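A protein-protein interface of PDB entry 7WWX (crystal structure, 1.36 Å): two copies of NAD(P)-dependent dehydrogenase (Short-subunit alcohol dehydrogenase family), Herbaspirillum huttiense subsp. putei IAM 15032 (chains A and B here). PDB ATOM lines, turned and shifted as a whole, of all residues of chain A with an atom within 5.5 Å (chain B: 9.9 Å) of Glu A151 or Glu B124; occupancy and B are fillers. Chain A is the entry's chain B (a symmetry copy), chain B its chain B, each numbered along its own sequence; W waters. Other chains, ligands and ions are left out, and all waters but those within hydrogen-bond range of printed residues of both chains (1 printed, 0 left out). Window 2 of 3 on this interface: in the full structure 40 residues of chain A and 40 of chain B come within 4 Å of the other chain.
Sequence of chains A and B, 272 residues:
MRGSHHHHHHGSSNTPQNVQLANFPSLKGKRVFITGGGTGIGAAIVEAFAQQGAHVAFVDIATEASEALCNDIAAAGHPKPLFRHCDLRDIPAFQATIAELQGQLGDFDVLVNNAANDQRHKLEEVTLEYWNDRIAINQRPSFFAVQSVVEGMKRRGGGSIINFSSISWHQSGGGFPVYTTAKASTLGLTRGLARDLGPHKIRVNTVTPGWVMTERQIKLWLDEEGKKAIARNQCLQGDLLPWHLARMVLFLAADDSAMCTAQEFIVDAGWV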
ATOM      1  N   ASP A 107      13.482 -23.359  17.892  1.00  0.00           N
ATOM      2  CA  ASP A 107      14.745 -22.901  17.259  1.00  0.00           C
ATOM      3  C   ASP A 107      14.771 -21.374  17.213  1.00  0.00           C
ATOM      4  O   ASP A 107      13.746 -20.715  16.942  1.00  0.00           O
ATOM      5  CB  ASP A 107      14.902 -23.510  15.872  1.00  0.00           C
ATOM      6  CG  ASP A 107      15.140 -25.013  15.957  1.00  0.00           C
ATOM      7  OD1 ASP A 107      15.738 -25.438  16.927  1.00  0.00           O
ATOM      8  OD2 ASP A 107      14.849 -25.695  14.961  1.00  0.00           O
ATOM      9  N   GLN A 147      27.632 -21.274  18.089  1.00  0.00           N
ATOM     10  CA  GLN A 147      27.651 -22.761  17.969  1.00  0.00           C
ATOM     11  C   GLN A 147      26.331 -23.386  18.459  1.00  0.00           C
ATOM     12  O   GLN A 147      25.833 -24.289  17.784  1.00  0.00           O
ATOM     13  CB  GLN A 147      28.856 -23.289  18.738  1.00  0.00           C
ATOM     14  CG  GLN A 147      29.024 -24.796  18.514  1.00  0.00           C
ATOM     15  CD  GLN A 147      30.168 -25.354  19.342  1.00  0.00           C
ATOM     16  OE1 GLN A 147      30.037 -25.505  20.547  1.00  0.00           O
ATOM     17  NE2 GLN A 147      31.300 -25.604  18.707  1.00  0.00           N
ATOM     18  N   SER A 148      25.785 -22.863  19.517  1.00  0.00           N
ATOM     19  CA  SER A 148      24.550 -23.368  20.140  1.00  0.00           C
ATOM     20  C   SER A 148      23.317 -23.042  19.311  1.00  0.00           C
ATOM     21  O   SER A 148      22.343 -23.793  19.472  1.00  0.00           O
ATOM     22  CB  SER A 148      24.401 -22.851  21.515  1.00  0.00           C
ATOM     23  OG  SER A 148      25.252 -23.493  22.408  1.00  0.00           O
ATOM     24  N   VAL A 149      23.263 -21.988  18.503  1.00  0.00           N
ATOM     25  CA  VAL A 149      22.003 -21.600  17.806  1.00  0.00           C
ATOM     26  C   VAL A 149      22.012 -22.040  16.359  1.00  0.00           C
ATOM     27  O   VAL A 149      20.930 -22.078  15.742  1.00  0.00           O
ATOM     28  CB  VAL A 149      21.674 -20.104  17.900  1.00  0.00           C
ATOM     29  CG1 VAL A 149      21.528 -19.674  19.352  1.00  0.00           C
ATOM     30  CG2 VAL A 149      22.641 -19.246  17.116  1.00  0.00           C
ATOM     31  N   VAL A 150      23.167 -22.356  15.768  1.00  0.00           N
ATOM     32  CA  VAL A 150      23.232 -22.489  14.290  1.00  0.00           C
ATOM     33  C   VAL A 150      22.394 -23.666  13.783  1.00  0.00           C
ATOM     34  O   VAL A 150      21.826 -23.537  12.694  1.00  0.00           O
ATOM     35  CB  VAL A 150      24.692 -22.563  13.793  1.00  0.00           C
ATOM     36  CG1 VAL A 150      25.446 -23.778  14.334  1.00  0.00           C
ATOM     37  CG2 VAL A 150      24.789 -22.574  12.297  1.00  0.00           C
ATOM     38  N   GLU A 151      22.343 -24.802  14.468  1.00  0.00           N
ATOM     39  CA  GLU A 151      21.604 -25.944  13.834  1.00  0.00           C
ATOM     40  C   GLU A 151      20.106 -25.617  13.764  1.00  0.00           C
ATOM     41  O   GLU A 151      19.473 -25.932  12.745  1.00  0.00           O
ATOM     42  CB  GLU A 151      21.893 -27.250  14.557  1.00  0.00           C
ATOM     43  CG  GLU A 151      23.295 -27.750  14.284  1.00  0.00           C
ATOM     44  CD  GLU A 151      23.639 -28.057  12.822  1.00  0.00           C
ATOM     45  OE1 GLU A 151      24.715 -27.664  12.404  1.00  0.00           O
ATOM     46  OE2 GLU A 151      22.847 -28.714  12.089  1.00  0.00           O
ATOM     47  N   GLY A 152      19.589 -24.902  14.755  1.00  0.00           N
ATOM     48  CA  GLY A 152      18.206 -24.446  14.742  1.00  0.00           C
ATOM     49  C   GLY A 152      17.973 -23.436  13.661  1.00  0.00           C
ATOM     50  O   GLY A 152      16.933 -23.449  13.020  1.00  0.00           O
ATOM     51  N   MET A 153      18.923 -22.500  13.461  1.00  0.00           N
ATOM     52  CA  MET A 153      18.749 -21.498  12.389  1.00  0.00           C
ATOM     53  C   MET A 153      18.724 -22.198  11.052  1.00  0.00           C
ATOM     54  O   MET A 153      17.923 -21.841  10.192  1.00  0.00           O
ATOM     55  CB  MET A 153      19.875 -20.454  12.386  1.00  0.00           C
ATOM     56  CG  MET A 153      19.761 -19.491  13.507  1.00  0.00           C
ATOM     57  SD  MET A 153      21.083 -18.260  13.382  1.00  0.00           S
ATOM     58  CE  MET A 153      20.624 -17.186  14.718  1.00  0.00           C
ATOM     59  N   LYS A 154      19.540 -23.244  10.872  1.00  0.00           N
ATOM     60  CA  LYS A 154      19.491 -23.985   9.579  1.00  0.00           C
ATOM     61  C   LYS A 154      18.104 -24.578   9.397  1.00  0.00           C
ATOM     62  O   LYS A 154      17.549 -24.485   8.295  1.00  0.00           O
ATOM     63  CB  LYS A 154      20.577 -25.051   9.523  1.00  0.00           C
ATOM     64  CG  LYS A 154      21.999 -24.535   9.459  1.00  0.00           C
ATOM     65  CD  LYS A 154      22.990 -25.690   9.516  1.00  0.00           C
ATOM     66  CE  LYS A 154      24.366 -25.288  10.001  1.00  0.00           C
ATOM     67  NZ  LYS A 154      25.251 -26.473  10.191  1.00  0.00           N
ATOM     68  N   ARG A 155      17.551 -25.134  10.452  1.00  0.00           N
ATOM     69  CA  ARG A 155      16.202 -25.764  10.386  1.00  0.00           C
ATOM     70  C   ARG A 155      15.158 -24.701  10.074  1.00  0.00           C
ATOM     71  O   ARG A 155      14.187 -25.006   9.328  1.00  0.00           O
ATOM     72  CB  ARG A 155      15.852 -26.490  11.681  1.00  0.00           C
ATOM     73  CG  ARG A 155      16.553 -27.830  11.863  1.00  0.00           C
ATOM     74  CD  ARG A 155      15.977 -28.558  13.067  1.00  0.00           C
ATOM     75  NE  ARG A 155      16.351 -27.959  14.346  1.00  0.00           N
ATOM     76  CZ  ARG A 155      17.421 -28.247  15.065  1.00  0.00           C
ATOM     77  NH1 ARG A 155      18.309 -29.143  14.652  1.00  0.00           N
ATOM     78  NH2 ARG A 155      17.626 -27.647  16.233  1.00  0.00           N
ATOM     79  N   ARG A 156      15.324 -23.472  10.583  1.00  0.00           N
ATOM     80  CA  ARG A 156      14.360 -22.378  10.332  1.00  0.00           C
ATOM     81  C   ARG A 156      14.550 -21.788   8.923  1.00  0.00           C
ATOM     82  O   ARG A 156      13.748 -20.948   8.559  1.00  0.00           O
ATOM     83  CB  ARG A 156      14.531 -21.295  11.408  1.00  0.00           C
ATOM     84  CG  ARG A 156      14.117 -21.749  12.804  1.00  0.00           C
ATOM     85  CD  ARG A 156      12.619 -21.873  12.995  1.00  0.00           C
ATOM     86  NE  ARG A 156      12.064 -20.556  13.234  1.00  0.00           N
ATOM     87  CZ  ARG A 156      10.781 -20.278  13.417  1.00  0.00           C
ATOM     88  NH1 ARG A 156      10.380 -19.036  13.632  1.00  0.00           N
ATOM     89  NH2 ARG A 156       9.890 -21.261  13.329  1.00  0.00           N
ATOM     90  N   LEU A 197      28.604 -19.350   7.202  1.00  0.00           N
ATOM     91  CA  LEU A 197      27.160 -19.537   7.469  1.00  0.00           C
ATOM     92  C   LEU A 197      26.299 -18.976   6.361  1.00  0.00           C
ATOM     93  O   LEU A 197      25.076 -19.276   6.330  1.00  0.00           O
ATOM     94  CB  LEU A 197      26.832 -18.911   8.827  1.00  0.00           C
ATOM     95  CG  LEU A 197      27.608 -19.476  10.015  1.00  0.00           C
ATOM     96  CD1 LEU A 197      27.173 -18.871  11.343  1.00  0.00           C
ATOM     97  CD2 LEU A 197      27.450 -21.020  10.030  1.00  0.00           C
ATOM     98  N   HIS A 200      23.800 -21.110   4.420  1.00  0.00           N
ATOM     99  CA  HIS A 200      22.591 -21.492   5.192  1.00  0.00           C
ATOM    100  C   HIS A 200      21.625 -20.302   5.305  1.00  0.00           C
ATOM    101  O   HIS A 200      20.635 -20.404   6.052  1.00  0.00           O
ATOM    102  CB  HIS A 200      23.018 -22.012   6.544  1.00  0.00           C
ATOM    103  CG  HIS A 200      24.001 -23.129   6.480  1.00  0.00           C
ATOM    104  ND1 HIS A 200      23.642 -24.359   5.936  1.00  0.00           N
ATOM    105  CD2 HIS A 200      25.291 -23.217   6.864  1.00  0.00           C
ATOM    106  CE1 HIS A 200      24.685 -25.162   6.018  1.00  0.00           C
ATOM    107  NE2 HIS A 200      25.719 -24.484   6.548  1.00  0.00           N
ATOM    108  N   HIS B 121      39.482 -25.191  10.964  1.00  0.00           N
ATOM    109  CA  HIS B 121      38.535 -25.771  11.930  1.00  0.00           C
ATOM    110  C   HIS B 121      37.133 -25.259  11.626  1.00  0.00           C
ATOM    111  O   HIS B 121      37.008 -24.173  11.055  1.00  0.00           O
ATOM    112  CB  HIS B 121      38.919 -25.435  13.366  1.00  0.00           C
ATOM    113  CG  HIS B 121      39.175 -23.975  13.594  1.00  0.00           C
ATOM    114  ND1 HIS B 121      40.447 -23.431  13.490  1.00  0.00           N
ATOM    115  CD2 HIS B 121      38.328 -22.953  13.872  1.00  0.00           C
ATOM    116  CE1 HIS B 121      40.348 -22.085  13.731  1.00  0.00           C
ATOM    117  NE2 HIS B 121      39.076 -21.795  13.986  1.00  0.00           N
ATOM    118  N   LYS B 122      36.130 -26.067  11.909  1.00  0.00           N
ATOM    119  CA  LYS B 122      34.729 -25.748  11.612  1.00  0.00           C
ATOM    120  C   LYS B 122      34.025 -25.364  12.905  1.00  0.00           C
ATOM    121  O   LYS B 122      34.234 -26.012  13.926  1.00  0.00           O
ATOM    122  CB  LYS B 122      34.068 -27.011  11.061  1.00  0.00           C
ATOM    123  CG  LYS B 122      34.243 -27.261   9.578  1.00  0.00           C
ATOM    124  CD  LYS B 122      33.363 -28.398   9.134  1.00  0.00           C
ATOM    125  CE  LYS B 122      31.907 -28.178   9.488  1.00  0.00           C
ATOM    126  NZ  LYS B 122      30.994 -28.886   8.555  1.00  0.00           N
ATOM    127  N   LEU B 123      33.220 -24.321  12.863  1.00  0.00           N
ATOM    128  CA  LEU B 123      32.379 -23.872  13.994  1.00  0.00           C
ATOM    129  C   LEU B 123      31.831 -25.059  14.784  1.00  0.00           C
ATOM    130  O   LEU B 123      31.961 -25.053  15.992  1.00  0.00           O
ATOM    131  CB  LEU B 123      31.229 -23.036  13.427  1.00  0.00           C
ATOM    132  CG  LEU B 123      30.127 -22.654  14.425  1.00  0.00           C
ATOM    133  CD1 LEU B 123      30.599 -21.714  15.524  1.00  0.00           C
ATOM    134  CD2 LEU B 123      28.911 -22.142  13.692  1.00  0.00           C
ATOM    135  N   GLU B 124      31.133 -25.963  14.096  1.00  0.00           N
ATOM    136  CA  GLU B 124      30.321 -27.027  14.725  1.00  0.00           C
ATOM    137  C   GLU B 124      31.220 -28.051  15.425  1.00  0.00           C
ATOM    138  O   GLU B 124      30.687 -28.812  16.283  1.00  0.00           O
ATOM    139  CB  GLU B 124      29.433 -27.683  13.656  1.00  0.00           C
ATOM    140  CG  GLU B 124      28.429 -26.725  13.022  1.00  0.00           C
ATOM    141  CD  GLU B 124      28.844 -25.909  11.798  1.00  0.00           C
ATOM    142  OE1 GLU B 124      30.077 -25.797  11.473  1.00  0.00           O
ATOM    143  OE2 GLU B 124      27.929 -25.422  11.124  1.00  0.00           O
ATOM    144  N   GLU B 125      32.524 -28.071  15.137  1.00  0.00           N
ATOM    145  CA  GLU B 125      33.443 -29.078  15.718  1.00  0.00           C
ATOM    146  C   GLU B 125      34.352 -28.517  16.814  1.00  0.00           C
ATOM    147  O   GLU B 125      35.052 -29.300  17.463  1.00  0.00           O
ATOM    148  CB  GLU B 125      34.239 -29.683  14.577  1.00  0.00           C
ATOM    149  CG  GLU B 125      33.332 -30.493  13.677  1.00  0.00           C
ATOM    150  CD  GLU B 125      33.979 -30.979  12.396  1.00  0.00           C
ATOM    151  OE1 GLU B 125      33.262 -31.654  11.620  1.00  0.00           O
ATOM    152  OE2 GLU B 125      35.166 -30.623  12.142  1.00  0.00           O
ATOM    153  N   VAL B 126      34.360 -27.198  17.040  1.00  0.00           N
ATOM    154  CA  VAL B 126      35.287 -26.561  17.997  1.00  0.00           C
ATOM    155  C   VAL B 126      34.827 -26.848  19.431  1.00  0.00           C
ATOM    156  O   VAL B 126      33.711 -26.492  19.815  1.00  0.00           O
ATOM    157  CB  VAL B 126      35.398 -25.063  17.683  1.00  0.00           C
ATOM    158  CG1 VAL B 126      36.020 -24.342  18.855  1.00  0.00           C
ATOM    159  CG2 VAL B 126      36.154 -24.827  16.393  1.00  0.00           C
ATOM    160  N   THR B 127      35.672 -27.518  20.226  1.00  0.00           N
ATOM    161  CA  THR B 127      35.390 -27.685  21.657  1.00  0.00           C
ATOM    162  C   THR B 127      35.876 -26.479  22.453  1.00  0.00           C
ATOM    163  O   THR B 127      36.723 -25.662  21.960  1.00  0.00           O
ATOM    164  CB  THR B 127      36.089 -28.927  22.199  1.00  0.00           C
ATOM    165  OG1 THR B 127      37.489 -28.705  22.022  1.00  0.00           O
ATOM    166  CG2 THR B 127      35.614 -30.165  21.488  1.00  0.00           C
ATOM    167  N   LEU B 128      35.450 -26.362  23.689  1.00  0.00           N
ATOM    168  CA  LEU B 128      35.980 -25.331  24.611  1.00  0.00           C
ATOM    169  C   LEU B 128      37.512 -25.410  24.658  1.00  0.00           C
ATOM    170  O   LEU B 128      38.224 -24.379  24.630  1.00  0.00           O
ATOM    171  CB  LEU B 128      35.378 -25.577  25.983  1.00  0.00           C
ATOM    172  CG  LEU B 128      35.880 -24.704  27.103  1.00  0.00           C
ATOM    173  CD1 LEU B 128      35.650 -23.221  26.795  1.00  0.00           C
ATOM    174  CD2 LEU B 128      35.182 -25.137  28.387  1.00  0.00           C
ATOM    175  N   TYR B 130      39.668 -26.675  22.497  1.00  0.00           N
ATOM    176  CA  TYR B 130      40.267 -26.261  21.210  1.00  0.00           C
ATOM    177  C   TYR B 130      40.220 -24.723  21.096  1.00  0.00           C
ATOM    178  O   TYR B 130      41.217 -24.100  20.721  1.00  0.00           O
ATOM    179  CB  TYR B 130      39.589 -26.938  20.026  1.00  0.00           C
ATOM    180  CG  TYR B 130      40.250 -26.686  18.714  1.00  0.00           C
ATOM    181  CD1 TYR B 130      41.409 -27.345  18.356  1.00  0.00           C
ATOM    182  CD2 TYR B 130      39.799 -25.673  17.893  1.00  0.00           C
ATOM    183  CE1 TYR B 130      42.033 -27.106  17.153  1.00  0.00           C
ATOM    184  CE2 TYR B 130      40.388 -25.458  16.676  1.00  0.00           C
ATOM    185  CZ  TYR B 130      41.511 -26.159  16.296  1.00  0.00           C
ATOM    186  OH  TYR B 130      42.084 -25.900  15.092  1.00  0.00           O
ATOM    187  N   GLY B 175      36.478 -21.151   6.932  1.00  0.00           N
ATOM    188  CA  GLY B 175      37.185 -22.384   7.329  1.00  0.00           C
ATOM    189  C   GLY B 175      38.040 -22.250   8.567  1.00  0.00           C
ATOM    190  O   GLY B 175      38.743 -23.221   8.867  1.00  0.00           O
ATOM    191  N   PHE B 176      38.046 -21.141   9.319  1.00  0.00           N
ATOM    192  CA  PHE B 176      38.839 -21.019  10.563  1.00  0.00           C
ATOM    193  C   PHE B 176      38.381 -19.834  11.406  1.00  0.00           C
ATOM    194  O   PHE B 176      39.146 -18.887  11.623  1.00  0.00           O
ATOM    195  CB  PHE B 176      40.345 -20.971  10.299  1.00  0.00           C
ATOM    196  CG  PHE B 176      40.895 -20.062   9.235  1.00  0.00           C
ATOM    197  CD1 PHE B 176      40.155 -19.041   8.644  1.00  0.00           C
ATOM    198  CD2 PHE B 176      42.195 -20.239   8.839  1.00  0.00           C
ATOM    199  CE1 PHE B 176      40.740 -18.207   7.694  1.00  0.00           C
ATOM    200  CE2 PHE B 176      42.780 -19.423   7.888  1.00  0.00           C
ATOM    201  CZ  PHE B 176      42.038 -18.425   7.303  1.00  0.00           C
ATOM    202  N   PRO B 177      37.131 -19.832  11.889  1.00  0.00           N
ATOM    203  CA  PRO B 177      36.580 -18.642  12.543  1.00  0.00           C
ATOM    204  C   PRO B 177      37.312 -18.223  13.799  1.00  0.00           C
ATOM    205  O   PRO B 177      37.261 -17.028  14.126  1.00  0.00           O
ATOM    206  CB  PRO B 177      35.123 -18.991  12.840  1.00  0.00           C
ATOM    207  CG  PRO B 177      35.142 -20.530  12.819  1.00  0.00           C
ATOM    208  CD  PRO B 177      36.117 -20.873  11.716  1.00  0.00           C
ATOM    209  N   VAL B 178      37.979 -19.113  14.528  1.00  0.00           N
ATOM    210  CA  VAL B 178      38.727 -18.709  15.752  1.00  0.00           C
ATOM    211  C   VAL B 178      39.996 -18.021  15.305  1.00  0.00           C
ATOM    212  O   VAL B 178      40.480 -17.080  16.016  1.00  0.00           O
ATOM    213  CB  VAL B 178      38.971 -19.871  16.735  1.00  0.00           C
ATOM    214  CG1 VAL B 178      39.486 -19.334  18.054  1.00  0.00           C
ATOM    215  CG2 VAL B 178      37.662 -20.627  16.933  1.00  0.00           C
HETATM  216  O   HOH W   1      28.315 -24.126   8.270  1.00  0.00           O
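NE2 of Gln A147 is in hydrogen-bond range of O of Leu B123.
The side-chain carboxylate of Glu B124 lies within salt-bridge range of the side-chain amino group of Lys A154, at 3.0 Å.
O of Val B126 lies within hydrogen-bond range of NE2 of Gln A147.
The side-chain carboxylate (OE1) of Glu A151 is in salt-bridge range of the side-chain amino group (NZ) of Lys A154 (2.6 Å).
Val A150 touches Leu B123 (CG1 to CD2, 3.9 Å).
Glu B124 touches Glu A151.
Of the printed residues of chain B, Gln A147 touches Leu B123 and Val B126.
No residue of chain B comes within 4 Å of Gly A152.
Of chain B, only Glu B124 (3.0 Å) comes within 4 Å of Lys A154.
Of the printed residues of chain A, Leu B123 touches Gln A147 (2.8 Å) and Val A150 (3.9 Å).
Glu B124 touches just these residues of chain A: Glu A151 (3.9 Å) and Lys A154 (3.0 Å).
Printed residues of chain A within 4 Å of Val B126: Gln A147 (2.8 Å).
Thr B127 touches none of the printed residues of chain A.
Leu B128 touches none of the printed residues of chain A.
The nearest residue of chain B that does not touch Glu A151 is Leu B123 (7.1 Å).
The nearest printed residue of chain A that does not touch Val B126 is Ser A148 (8.7 Å).
Of the 13 printed residues of chain B, 3 touch a printed residue of chain A.
Hydrophobic or aromatic side chains of chain B that line the printed part of chain A: Leu B123.
Hydrophobic or aromatic side chains of chain A within 4 Å of the printed part of chain B: Val A150.
Among the printed residues, Asp or Glu carboxylates within 4 Å of a Lys or Arg side-chain nitrogen of the other chain: Lys A154 with Glu B124.
No position is printed for both chains.
Water W1 bridges a ring nitrogen (NE2) of His A200 (3.1 Å) and the side-chain carboxylate (OE2) of Glu B124 (3.2 Å).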
